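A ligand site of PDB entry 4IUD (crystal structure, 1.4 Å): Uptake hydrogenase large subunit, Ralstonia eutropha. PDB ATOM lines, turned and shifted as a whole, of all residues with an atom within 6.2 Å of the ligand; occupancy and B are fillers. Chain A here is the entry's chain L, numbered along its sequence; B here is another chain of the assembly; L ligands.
The side-chain sulfur (SG) of Cys 600 binds an iron atom (FE1) of the ligand, at 2.4 Å. The side-chain sulfur of Cys 75 is bound to a nickel atom (NI1) of the ligand, 2.2 Å away. The backbone NH (N) of Thr 553 lies within hydrogen-bond range of a nitrogen (N1) of the ligand (2.9 Å). The guanidinium group (NH1) of Arg 530 lies within hydrogen-bond range of a nitrogen (N2) of the ligand (3.3 Å). The side-chain sulfur (SG) of Cys 81 is in hydrogen-bond range of an oxygen (O1) of the ligand. The side-chain hydroxyl of Thr 553 is in hydrogen-bond range of a nitrogen (N1) of the ligand, at 2.9 Å. The side-chain sulfur (SG) of Cys 78 binds an iron atom (FE1) of the ligand (2.4 Å). An oxygen (O1) of the ligand is in hydrogen-bond range of a ring nitrogen (NE2) of His 82 (3.2 Å). SG of CSO 597 binds a nickel atom (NI1) of the ligand (2.3 Å). N2 of the ligand is in hydrogen-bond range of N of Arg 530 (2.9 Å).
The side-chain hydroxyl (OG1) of Thr 553 sits at hydrogen-bond distance from N of CSO 597 (3.2 Å). NH2 of Arg 530 is in salt-bridge range of OD1 of Asp 595 (2.9 Å). The backbone carbonyl oxygen (O) of Val 551 sits close to the side-chain hydroxyl (OG1) of Thr 554 (3.2 Å). O of Cys 78 sits at hydrogen-bond distance from SG of Cys 81, 3.2 Å away. The backbone NH of Val 77 lies close to the side-chain sulfur of Cys 75 (3.4 Å). A ring nitrogen (ND1) of His 82 lies within hydrogen-bond range of a ring nitrogen (NE2) of His 535 (3.0 Å). The side-chain sulfur (SG) of Cys 600 lies close to a ring nitrogen (NE2) of His 82 (3.2 Å). The guanidinium group (NH2) of Arg 530 lies within salt-bridge range of the side-chain carboxylate (OD1) of Asp 117 (2.7 Å).
A nitrogen (N2) of the ligand lies close to the backbone nitrogen (N) of Pro 529, at 3.2 Å. Residues that only touch the ligand: Ala 528 (3.4 Å), Leu 533 (3.3 Å), Val 551 (3.3 Å) and Pro 552 (3.4 Å). Within 4 Å of the ligand: Cys 75, Cys 78, Cys 81, His 82, Ala 528, Pro 529, Arg 530, Leu 533, Val 551, Pro 552, Thr 553, CSO 597 and Cys 600. The nearest printed residue that does not touch the ligand is Val 77 (4.5 Å).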
ATOM      1  N   GLU A  27     -17.144   1.438  21.221  1.00  0.00           N
ATOM      2  CA  GLU A  27     -16.773   0.713  20.004  1.00  0.00           C
ATOM      3  C   GLU A  27     -17.025  -0.756  20.253  1.00  0.00           C
ATOM      4  O   GLU A  27     -16.632  -1.295  21.283  1.00  0.00           O
ATOM      5  CB  GLU A  27     -15.310   0.947  19.627  1.00  0.00           C
ATOM      6  CG  GLU A  27     -14.930   0.365  18.253  1.00  0.00           C
ATOM      7  CD  GLU A  27     -14.916  -1.166  18.200  1.00  0.00           C
ATOM      8  OE1 GLU A  27     -14.648  -1.807  19.235  1.00  0.00           O
ATOM      9  OE2 GLU A  27     -15.190  -1.738  17.121  1.00  0.00           O
ATOM     10  N   ILE A  74      -7.541  -4.254  13.671  1.00  0.00           N
ATOM     11  CA  ILE A  74      -8.123  -4.544  14.976  1.00  0.00           C
ATOM     12  C   ILE A  74      -9.124  -3.441  15.350  1.00  0.00           C
ATOM     13  O   ILE A  74     -10.162  -3.711  15.969  1.00  0.00           O
ATOM     14  CB  ILE A  74      -7.050  -4.684  16.074  1.00  0.00           C
ATOM     15  CG1 ILE A  74      -6.289  -5.992  15.879  1.00  0.00           C
ATOM     16  CG2 ILE A  74      -7.688  -4.625  17.460  1.00  0.00           C
ATOM     17  CD1 ILE A  74      -5.075  -6.156  16.763  1.00  0.00           C
ATOM     18  N   CYS A  75      -8.839  -2.205  14.951  1.00  0.00           N
ATOM     19  CA  CYS A  75      -9.665  -1.094  15.367  1.00  0.00           C
ATOM     20  C   CYS A  75      -9.510   0.154  14.504  1.00  0.00           C
ATOM     21  O   CYS A  75      -8.411   0.623  14.265  1.00  0.00           O
ATOM     22  CB  CYS A  75      -9.360  -0.727  16.801  1.00  0.00           C
ATOM     23  SG  CYS A  75     -10.609   0.367  17.463  1.00  0.00           S
ATOM     24  N   GLY A  76     -10.649   0.672  14.045  1.00  0.00           N
ATOM     25  CA  GLY A  76     -10.690   1.904  13.237  1.00  0.00           C
ATOM     26  C   GLY A  76     -10.924   3.169  14.047  1.00  0.00           C
ATOM     27  O   GLY A  76     -10.926   4.263  13.478  1.00  0.00           O
ATOM     28  N   VAL A  77     -11.155   3.025  15.352  1.00  0.00           N
ATOM     29  CA  VAL A  77     -11.326   4.166  16.239  1.00  0.00           C
ATOM     30  C   VAL A  77      -9.951   4.588  16.729  1.00  0.00           C
ATOM     31  O   VAL A  77      -9.524   5.716  16.518  1.00  0.00           O
ATOM     32  CB  VAL A  77     -12.266   3.844  17.428  1.00  0.00           C
ATOM     33  CG1 VAL A  77     -12.390   5.032  18.371  1.00  0.00           C
ATOM     34  CG2 VAL A  77     -13.631   3.424  16.902  1.00  0.00           C
ATOM     35  N   CYS A  78      -9.237   3.660  17.363  1.00  0.00           N
ATOM     36  CA  CYS A  78      -7.834   3.893  17.705  1.00  0.00           C
ATOM     37  C   CYS A  78      -6.959   3.549  16.492  1.00  0.00           C
ATOM     38  O   CYS A  78      -5.998   2.779  16.577  1.00  0.00           O
ATOM     39  CB  CYS A  78      -7.421   3.134  18.981  1.00  0.00           C
ATOM     40  SG  CYS A  78      -7.579   1.324  18.964  1.00  0.00           S
ATOM     41  N   THR A  79      -7.308   4.141  15.360  1.00  0.00           N
ATOM     42  CA  THR A  79      -6.703   3.760  14.101  1.00  0.00           C
ATOM     43  C   THR A  79      -5.226   4.179  14.000  1.00  0.00           C
ATOM     44  O   THR A  79      -4.872   5.353  14.157  1.00  0.00           O
ATOM     45  CB  THR A  79      -7.507   4.316  12.898  1.00  0.00           C
ATOM     46  OG1 THR A  79      -6.909   3.854  11.687  1.00  0.00           O
ATOM     47  CG2 THR A  79      -7.542   5.848  12.907  1.00  0.00           C
ATOM     48  N   CYS A  81      -2.705   2.977  15.997  1.00  0.00           N
ATOM     49  CA  CYS A  81      -1.900   2.629  17.178  1.00  0.00           C
ATOM     50  C   CYS A  81      -1.435   1.176  17.111  1.00  0.00           C
ATOM     51  O   CYS A  81      -0.315   0.876  17.527  1.00  0.00           O
ATOM     52  CB  CYS A  81      -2.632   2.944  18.498  1.00  0.00           C
ATOM     53  SG  CYS A  81      -4.022   1.884  18.949  1.00  0.00           S
ATOM     54  N   HIS A  82      -2.258   0.289  16.576  1.00  0.00           N
ATOM     55  CA  HIS A  82      -1.821  -1.114  16.369  1.00  0.00           C
ATOM     56  C   HIS A  82      -0.774  -1.220  15.293  1.00  0.00           C
ATOM     57  O   HIS A  82       0.127  -2.064  15.379  1.00  0.00           O
ATOM     58  CB  HIS A  82      -2.998  -2.016  16.043  1.00  0.00           C
ATOM     59  CG  HIS A  82      -3.913  -2.250  17.216  1.00  0.00           C
ATOM     60  ND1 HIS A  82      -3.572  -3.031  18.263  1.00  0.00           N
ATOM     61  CD2 HIS A  82      -5.164  -1.748  17.501  1.00  0.00           C
ATOM     62  CE1 HIS A  82      -4.571  -3.049  19.156  1.00  0.00           C
ATOM     63  NE2 HIS A  82      -5.550  -2.268  18.700  1.00  0.00           N
ATOM     64  N   LEU A 113      -3.864  11.089  16.797  1.00  0.00           N
ATOM     65  CA  LEU A 113      -4.848  10.061  17.180  1.00  0.00           C
ATOM     66  C   LEU A 113      -5.365  10.309  18.613  1.00  0.00           C
ATOM     67  O   LEU A 113      -6.566  10.248  18.845  1.00  0.00           O
ATOM     68  CB  LEU A 113      -4.268   8.650  17.066  1.00  0.00           C
ATOM     69  CG  LEU A 113      -5.222   7.527  17.510  1.00  0.00           C
ATOM     70  CD1 LEU A 113      -6.423   7.481  16.581  1.00  0.00           C
ATOM     71  CD2 LEU A 113      -4.517   6.178  17.564  1.00  0.00           C
ATOM     72  N   ASP A 117      -9.256  10.876  19.081  1.00  0.00           N
ATOM     73  CA  ASP A 117      -9.937   9.831  19.824  1.00  0.00           C
ATOM     74  C   ASP A 117     -10.558  10.388  21.125  1.00  0.00           C
ATOM     75  O   ASP A 117     -11.742  10.167  21.402  1.00  0.00           O
ATOM     76  CB  ASP A 117      -8.944   8.702  20.112  1.00  0.00           C
ATOM     77  CG  ASP A 117      -9.591   7.355  20.255  1.00  0.00           C
ATOM     78  OD1 ASP A 117     -10.734   7.299  20.737  1.00  0.00           O
ATOM     79  OD2 ASP A 117      -8.943   6.348  19.900  1.00  0.00           O
ATOM     80  N   ALA A 528      -1.433   3.842  23.878  1.00  0.00           N
ATOM     81  CA  ALA A 528      -2.603   4.051  23.032  1.00  0.00           C
ATOM     82  C   ALA A 528      -3.609   4.910  23.792  1.00  0.00           C
ATOM     83  O   ALA A 528      -3.500   5.060  25.015  1.00  0.00           O
ATOM     84  CB  ALA A 528      -3.213   2.710  22.662  1.00  0.00           C
ATOM     85  N   PRO A 529      -4.596   5.493  23.082  1.00  0.00           N
ATOM     86  CA  PRO A 529      -5.556   6.376  23.747  1.00  0.00           C
ATOM     87  C   PRO A 529      -6.193   5.782  25.017  1.00  0.00           C
ATOM     88  O   PRO A 529      -6.411   6.518  25.970  1.00  0.00           O
ATOM     89  CB  PRO A 529      -6.605   6.613  22.656  1.00  0.00           C
ATOM     90  CG  PRO A 529      -5.797   6.593  21.393  1.00  0.00           C
ATOM     91  CD  PRO A 529      -4.739   5.537  21.609  1.00  0.00           C
ATOM     92  N   ARG A 530      -6.446   4.478  25.033  1.00  0.00           N
ATOM     93  CA  ARG A 530      -7.126   3.836  26.160  1.00  0.00           C
ATOM     94  C   ARG A 530      -6.207   3.185  27.192  1.00  0.00           C
ATOM     95  O   ARG A 530      -6.681   2.665  28.198  1.00  0.00           O
ATOM     96  CB  ARG A 530      -8.149   2.829  25.653  1.00  0.00           C
ATOM     97  CG  ARG A 530      -9.333   3.498  24.991  1.00  0.00           C
ATOM     98  CD  ARG A 530     -10.002   2.628  23.964  1.00  0.00           C
ATOM     99  NE  ARG A 530     -10.978   3.408  23.216  1.00  0.00           N
ATOM    100  CZ  ARG A 530     -10.708   4.219  22.184  1.00  0.00           C
ATOM    101  NH1 ARG A 530      -9.470   4.342  21.721  1.00  0.00           N
ATOM    102  NH2 ARG A 530     -11.694   4.887  21.603  1.00  0.00           N
ATOM    103  N   GLY A 531      -4.889   3.235  26.975  1.00  0.00           N
ATOM    104  CA  GLY A 531      -3.928   2.714  27.951  1.00  0.00           C
ATOM    105  C   GLY A 531      -2.786   1.961  27.313  1.00  0.00           C
ATOM    106  O   GLY A 531      -2.303   2.318  26.242  1.00  0.00           O
ATOM    107  N   LEU A 533      -0.744  -0.635  25.399  1.00  0.00           N
ATOM    108  CA  LEU A 533      -0.821  -1.562  24.275  1.00  0.00           C
ATOM    109  C   LEU A 533       0.527  -2.233  24.055  1.00  0.00           C
ATOM    110  O   LEU A 533       1.554  -1.564  24.044  1.00  0.00           O
ATOM    111  CB  LEU A 533      -1.219  -0.807  22.991  1.00  0.00           C
ATOM    112  CG  LEU A 533      -1.172  -1.592  21.673  1.00  0.00           C
ATOM    113  CD1 LEU A 533      -2.088  -2.806  21.734  1.00  0.00           C
ATOM    114  CD2 LEU A 533      -1.506  -0.712  20.477  1.00  0.00           C
ATOM    115  N   HIS A 535       2.332  -5.487  21.443  1.00  0.00           N
ATOM    116  CA  HIS A 535       2.331  -6.569  20.467  1.00  0.00           C
ATOM    117  C   HIS A 535       3.603  -7.334  20.659  1.00  0.00           C
ATOM    118  O   HIS A 535       4.679  -6.729  20.705  1.00  0.00           O
ATOM    119  CB  HIS A 535       2.320  -6.024  19.052  1.00  0.00           C
ATOM    120  CG  HIS A 535       1.009  -5.430  18.591  1.00  0.00           C
ATOM    121  ND1 HIS A 535       0.714  -5.298  17.288  1.00  0.00           N
ATOM    122  CD2 HIS A 535      -0.072  -4.894  19.302  1.00  0.00           C
ATOM    123  CE1 HIS A 535      -0.500  -4.722  17.160  1.00  0.00           C
ATOM    124  NE2 HIS A 535      -0.979  -4.475  18.385  1.00  0.00           N
ATOM    125  N   VAL A 551      -4.124  -5.547  24.784  1.00  0.00           N
ATOM    126  CA  VAL A 551      -4.624  -4.255  24.331  1.00  0.00           C
ATOM    127  C   VAL A 551      -5.244  -3.539  25.555  1.00  0.00           C
ATOM    128  O   VAL A 551      -5.631  -4.200  26.508  1.00  0.00           O
ATOM    129  CB  VAL A 551      -5.607  -4.492  23.168  1.00  0.00           C
ATOM    130  CG1 VAL A 551      -6.057  -3.209  22.522  1.00  0.00           C
ATOM    131  CG2 VAL A 551      -4.962  -5.399  22.129  1.00  0.00           C
ATOM    132  N   PRO A 552      -5.314  -2.198  25.547  1.00  0.00           N
ATOM    133  CA  PRO A 552      -5.726  -1.528  26.779  1.00  0.00           C
ATOM    134  C   PRO A 552      -7.077  -1.982  27.321  1.00  0.00           C
ATOM    135  O   PRO A 552      -7.205  -2.218  28.521  1.00  0.00           O
ATOM    136  CB  PRO A 552      -5.772  -0.057  26.379  1.00  0.00           C
ATOM    137  CG  PRO A 552      -4.767   0.063  25.280  1.00  0.00           C
ATOM    138  CD  PRO A 552      -4.783  -1.246  24.550  1.00  0.00           C
ATOM    139  N   THR A 553      -8.073  -2.135  26.451  1.00  0.00           N
ATOM    140  CA  THR A 553      -9.396  -2.555  26.894  1.00  0.00           C
ATOM    141  C   THR A 553      -9.395  -4.053  27.284  1.00  0.00           C
ATOM    142  O   THR A 553     -10.264  -4.502  28.024  1.00  0.00           O
ATOM    143  CB  THR A 553     -10.508  -2.202  25.867  1.00  0.00           C
ATOM    144  OG1 THR A 553     -10.472  -0.786  25.613  1.00  0.00           O
ATOM    145  CG2 THR A 553     -11.897  -2.543  26.429  1.00  0.00           C
ATOM    146  N   THR A 554      -8.387  -4.815  26.838  1.00  0.00           N
ATOM    147  CA  THR A 554      -8.191  -6.176  27.374  1.00  0.00           C
ATOM    148  C   THR A 554      -7.927  -6.083  28.881  1.00  0.00           C
ATOM    149  O   THR A 554      -8.535  -6.815  29.650  1.00  0.00           O
ATOM    150  CB  THR A 554      -7.038  -6.957  26.707  1.00  0.00           C
ATOM    151  OG1 THR A 554      -7.073  -6.758  25.274  1.00  0.00           O
ATOM    152  CG2 THR A 554      -7.142  -8.439  27.021  1.00  0.00           C
ATOM    153  N   ASP A 595     -13.650   4.630  28.077  1.00  0.00           N
ATOM    154  CA  ASP A 595     -13.646   4.635  26.618  1.00  0.00           C
ATOM    155  C   ASP A 595     -13.465   3.193  26.096  1.00  0.00           C
ATOM    156  O   ASP A 595     -12.507   2.889  25.383  1.00  0.00           O
ATOM    157  CB  ASP A 595     -12.551   5.599  26.146  1.00  0.00           C
ATOM    158  CG  ASP A 595     -12.506   5.803  24.656  1.00  0.00           C
ATOM    159  OD1 ASP A 595     -13.427   5.391  23.924  1.00  0.00           O
ATOM    160  OD2 ASP A 595     -11.517   6.406  24.199  1.00  0.00           O
ATOM    161  N   PRO A 596     -14.385   2.288  26.461  1.00  0.00           N
ATOM    162  CA  PRO A 596     -14.209   0.896  26.063  1.00  0.00           C
ATOM    163  C   PRO A 596     -14.159   0.695  24.544  1.00  0.00           C
ATOM    164  O   PRO A 596     -15.029   1.205  23.814  1.00  0.00           O
ATOM    165  CB  PRO A 596     -15.469   0.206  26.641  1.00  0.00           C
ATOM    166  CG  PRO A 596     -15.965   1.126  27.707  1.00  0.00           C
ATOM    167  CD  PRO A 596     -15.647   2.495  27.189  1.00  0.00           C
ATOM    168  N   CSO A 597     -13.146  -0.020  24.082  1.00  0.00           N
ATOM    169  CA  CSO A 597     -13.050  -0.438  22.683  1.00  0.00           C
ATOM    170  CB  CSO A 597     -11.807   0.086  22.003  1.00  0.00           C
ATOM    171  SG  CSO A 597     -11.816  -0.405  20.297  1.00  0.00           S
ATOM    172  C   CSO A 597     -13.045  -1.940  22.676  1.00  0.00           C
ATOM    173  O   CSO A 597     -12.036  -2.569  22.984  1.00  0.00           O
ATOM    174  OD  CSO A 597     -12.283   1.110  19.607  1.00  0.00           O
ATOM    175  N   LEU A 598     -14.180  -2.519  22.333  1.00  0.00           N
ATOM    176  CA  LEU A 598     -14.344  -3.961  22.476  1.00  0.00           C
ATOM    177  C   LEU A 598     -13.691  -4.741  21.339  1.00  0.00           C
ATOM    178  O   LEU A 598     -13.222  -5.867  21.569  1.00  0.00           O
ATOM    179  CB  LEU A 598     -15.824  -4.315  22.642  1.00  0.00           C
ATOM    180  CG  LEU A 598     -16.343  -4.174  24.089  1.00  0.00           C
ATOM    181  CD1 LEU A 598     -15.807  -5.316  24.953  1.00  0.00           C
ATOM    182  CD2 LEU A 598     -16.005  -2.838  24.731  1.00  0.00           C
ATOM    183  N   ALA A 599     -13.622  -4.156  20.145  1.00  0.00           N
ATOM    184  CA  ALA A 599     -12.878  -4.780  19.039  1.00  0.00           C
ATOM    185  C   ALA A 599     -11.392  -4.905  19.414  1.00  0.00           C
ATOM    186  O   ALA A 599     -10.775  -5.940  19.205  1.00  0.00           O
ATOM    187  CB  ALA A 599     -13.057  -3.988  17.748  1.00  0.00           C
ATOM    188  N   CYS A 600     -10.841  -3.835  19.992  1.00  0.00           N
ATOM    189  CA  CYS A 600      -9.484  -3.869  20.540  1.00  0.00           C
ATOM    190  C   CYS A 600      -9.310  -4.931  21.594  1.00  0.00           C
ATOM    191  O   CYS A 600      -8.324  -5.659  21.585  1.00  0.00           O
ATOM    192  CB  CYS A 600      -9.131  -2.537  21.175  1.00  0.00           C
ATOM    193  SG  CYS A 600      -8.357  -1.383  20.057  1.00  0.00           S
ATOM    194  N   SER A 601     -10.267  -4.999  22.520  1.00  0.00           N
ATOM    195  CA  SER A 601     -10.115  -5.855  23.696  1.00  0.00           C
ATOM    196  C   SER A 601      -9.998  -7.332  23.335  1.00  0.00           C
ATOM    197  O   SER A 601      -9.289  -8.073  24.014  1.00  0.00           O
ATOM    198  CB  SER A 601     -11.278  -5.659  24.675  1.00  0.00           C
ATOM    199  OG  SER A 601     -12.470  -6.280  24.213  1.00  0.00           O
ATOM    200  N   CYS B  17     -14.224  -3.414  12.874  1.00  0.00           N
ATOM    201  CA  CYS B  17     -13.285  -2.570  13.602  1.00  0.00           C
ATOM    202  C   CYS B  17     -13.796  -1.128  13.745  1.00  0.00           C
ATOM    203  O   CYS B  17     -13.130  -0.299  14.355  1.00  0.00           O
ATOM    204  CB  CYS B  17     -11.940  -2.525  12.886  1.00  0.00           C
ATOM    205  SG  CYS B  17     -11.805  -1.256  11.616  1.00  0.00           S
HETATM  206 FE1  LIG L   1      -7.519   0.529  21.179  1.00  0.00          FE
HETATM  207 NI1  LIG L   1      -9.878   0.614  19.525  1.00  0.00          NI
HETATM  208  C1  LIG L   1      -5.794  -0.126  21.179  1.00  0.00           C
HETATM  209  O1  LIG L   1      -4.714  -0.528  21.205  1.00  0.00           O
HETATM  210  C2  LIG L   1      -7.929  -0.231  22.900  1.00  0.00           C
HETATM  211  N1  LIG L   1      -8.177  -0.686  23.897  1.00  0.00           N
HETATM  212  C3  LIG L   1      -6.923   2.148  22.025  1.00  0.00           C
HETATM  213  N2  LIG L   1      -6.562   3.074  22.485  1.00  0.00           N
HETATM  214  O2  LIG L   1      -9.376   1.280  21.193  1.00  0.00           O
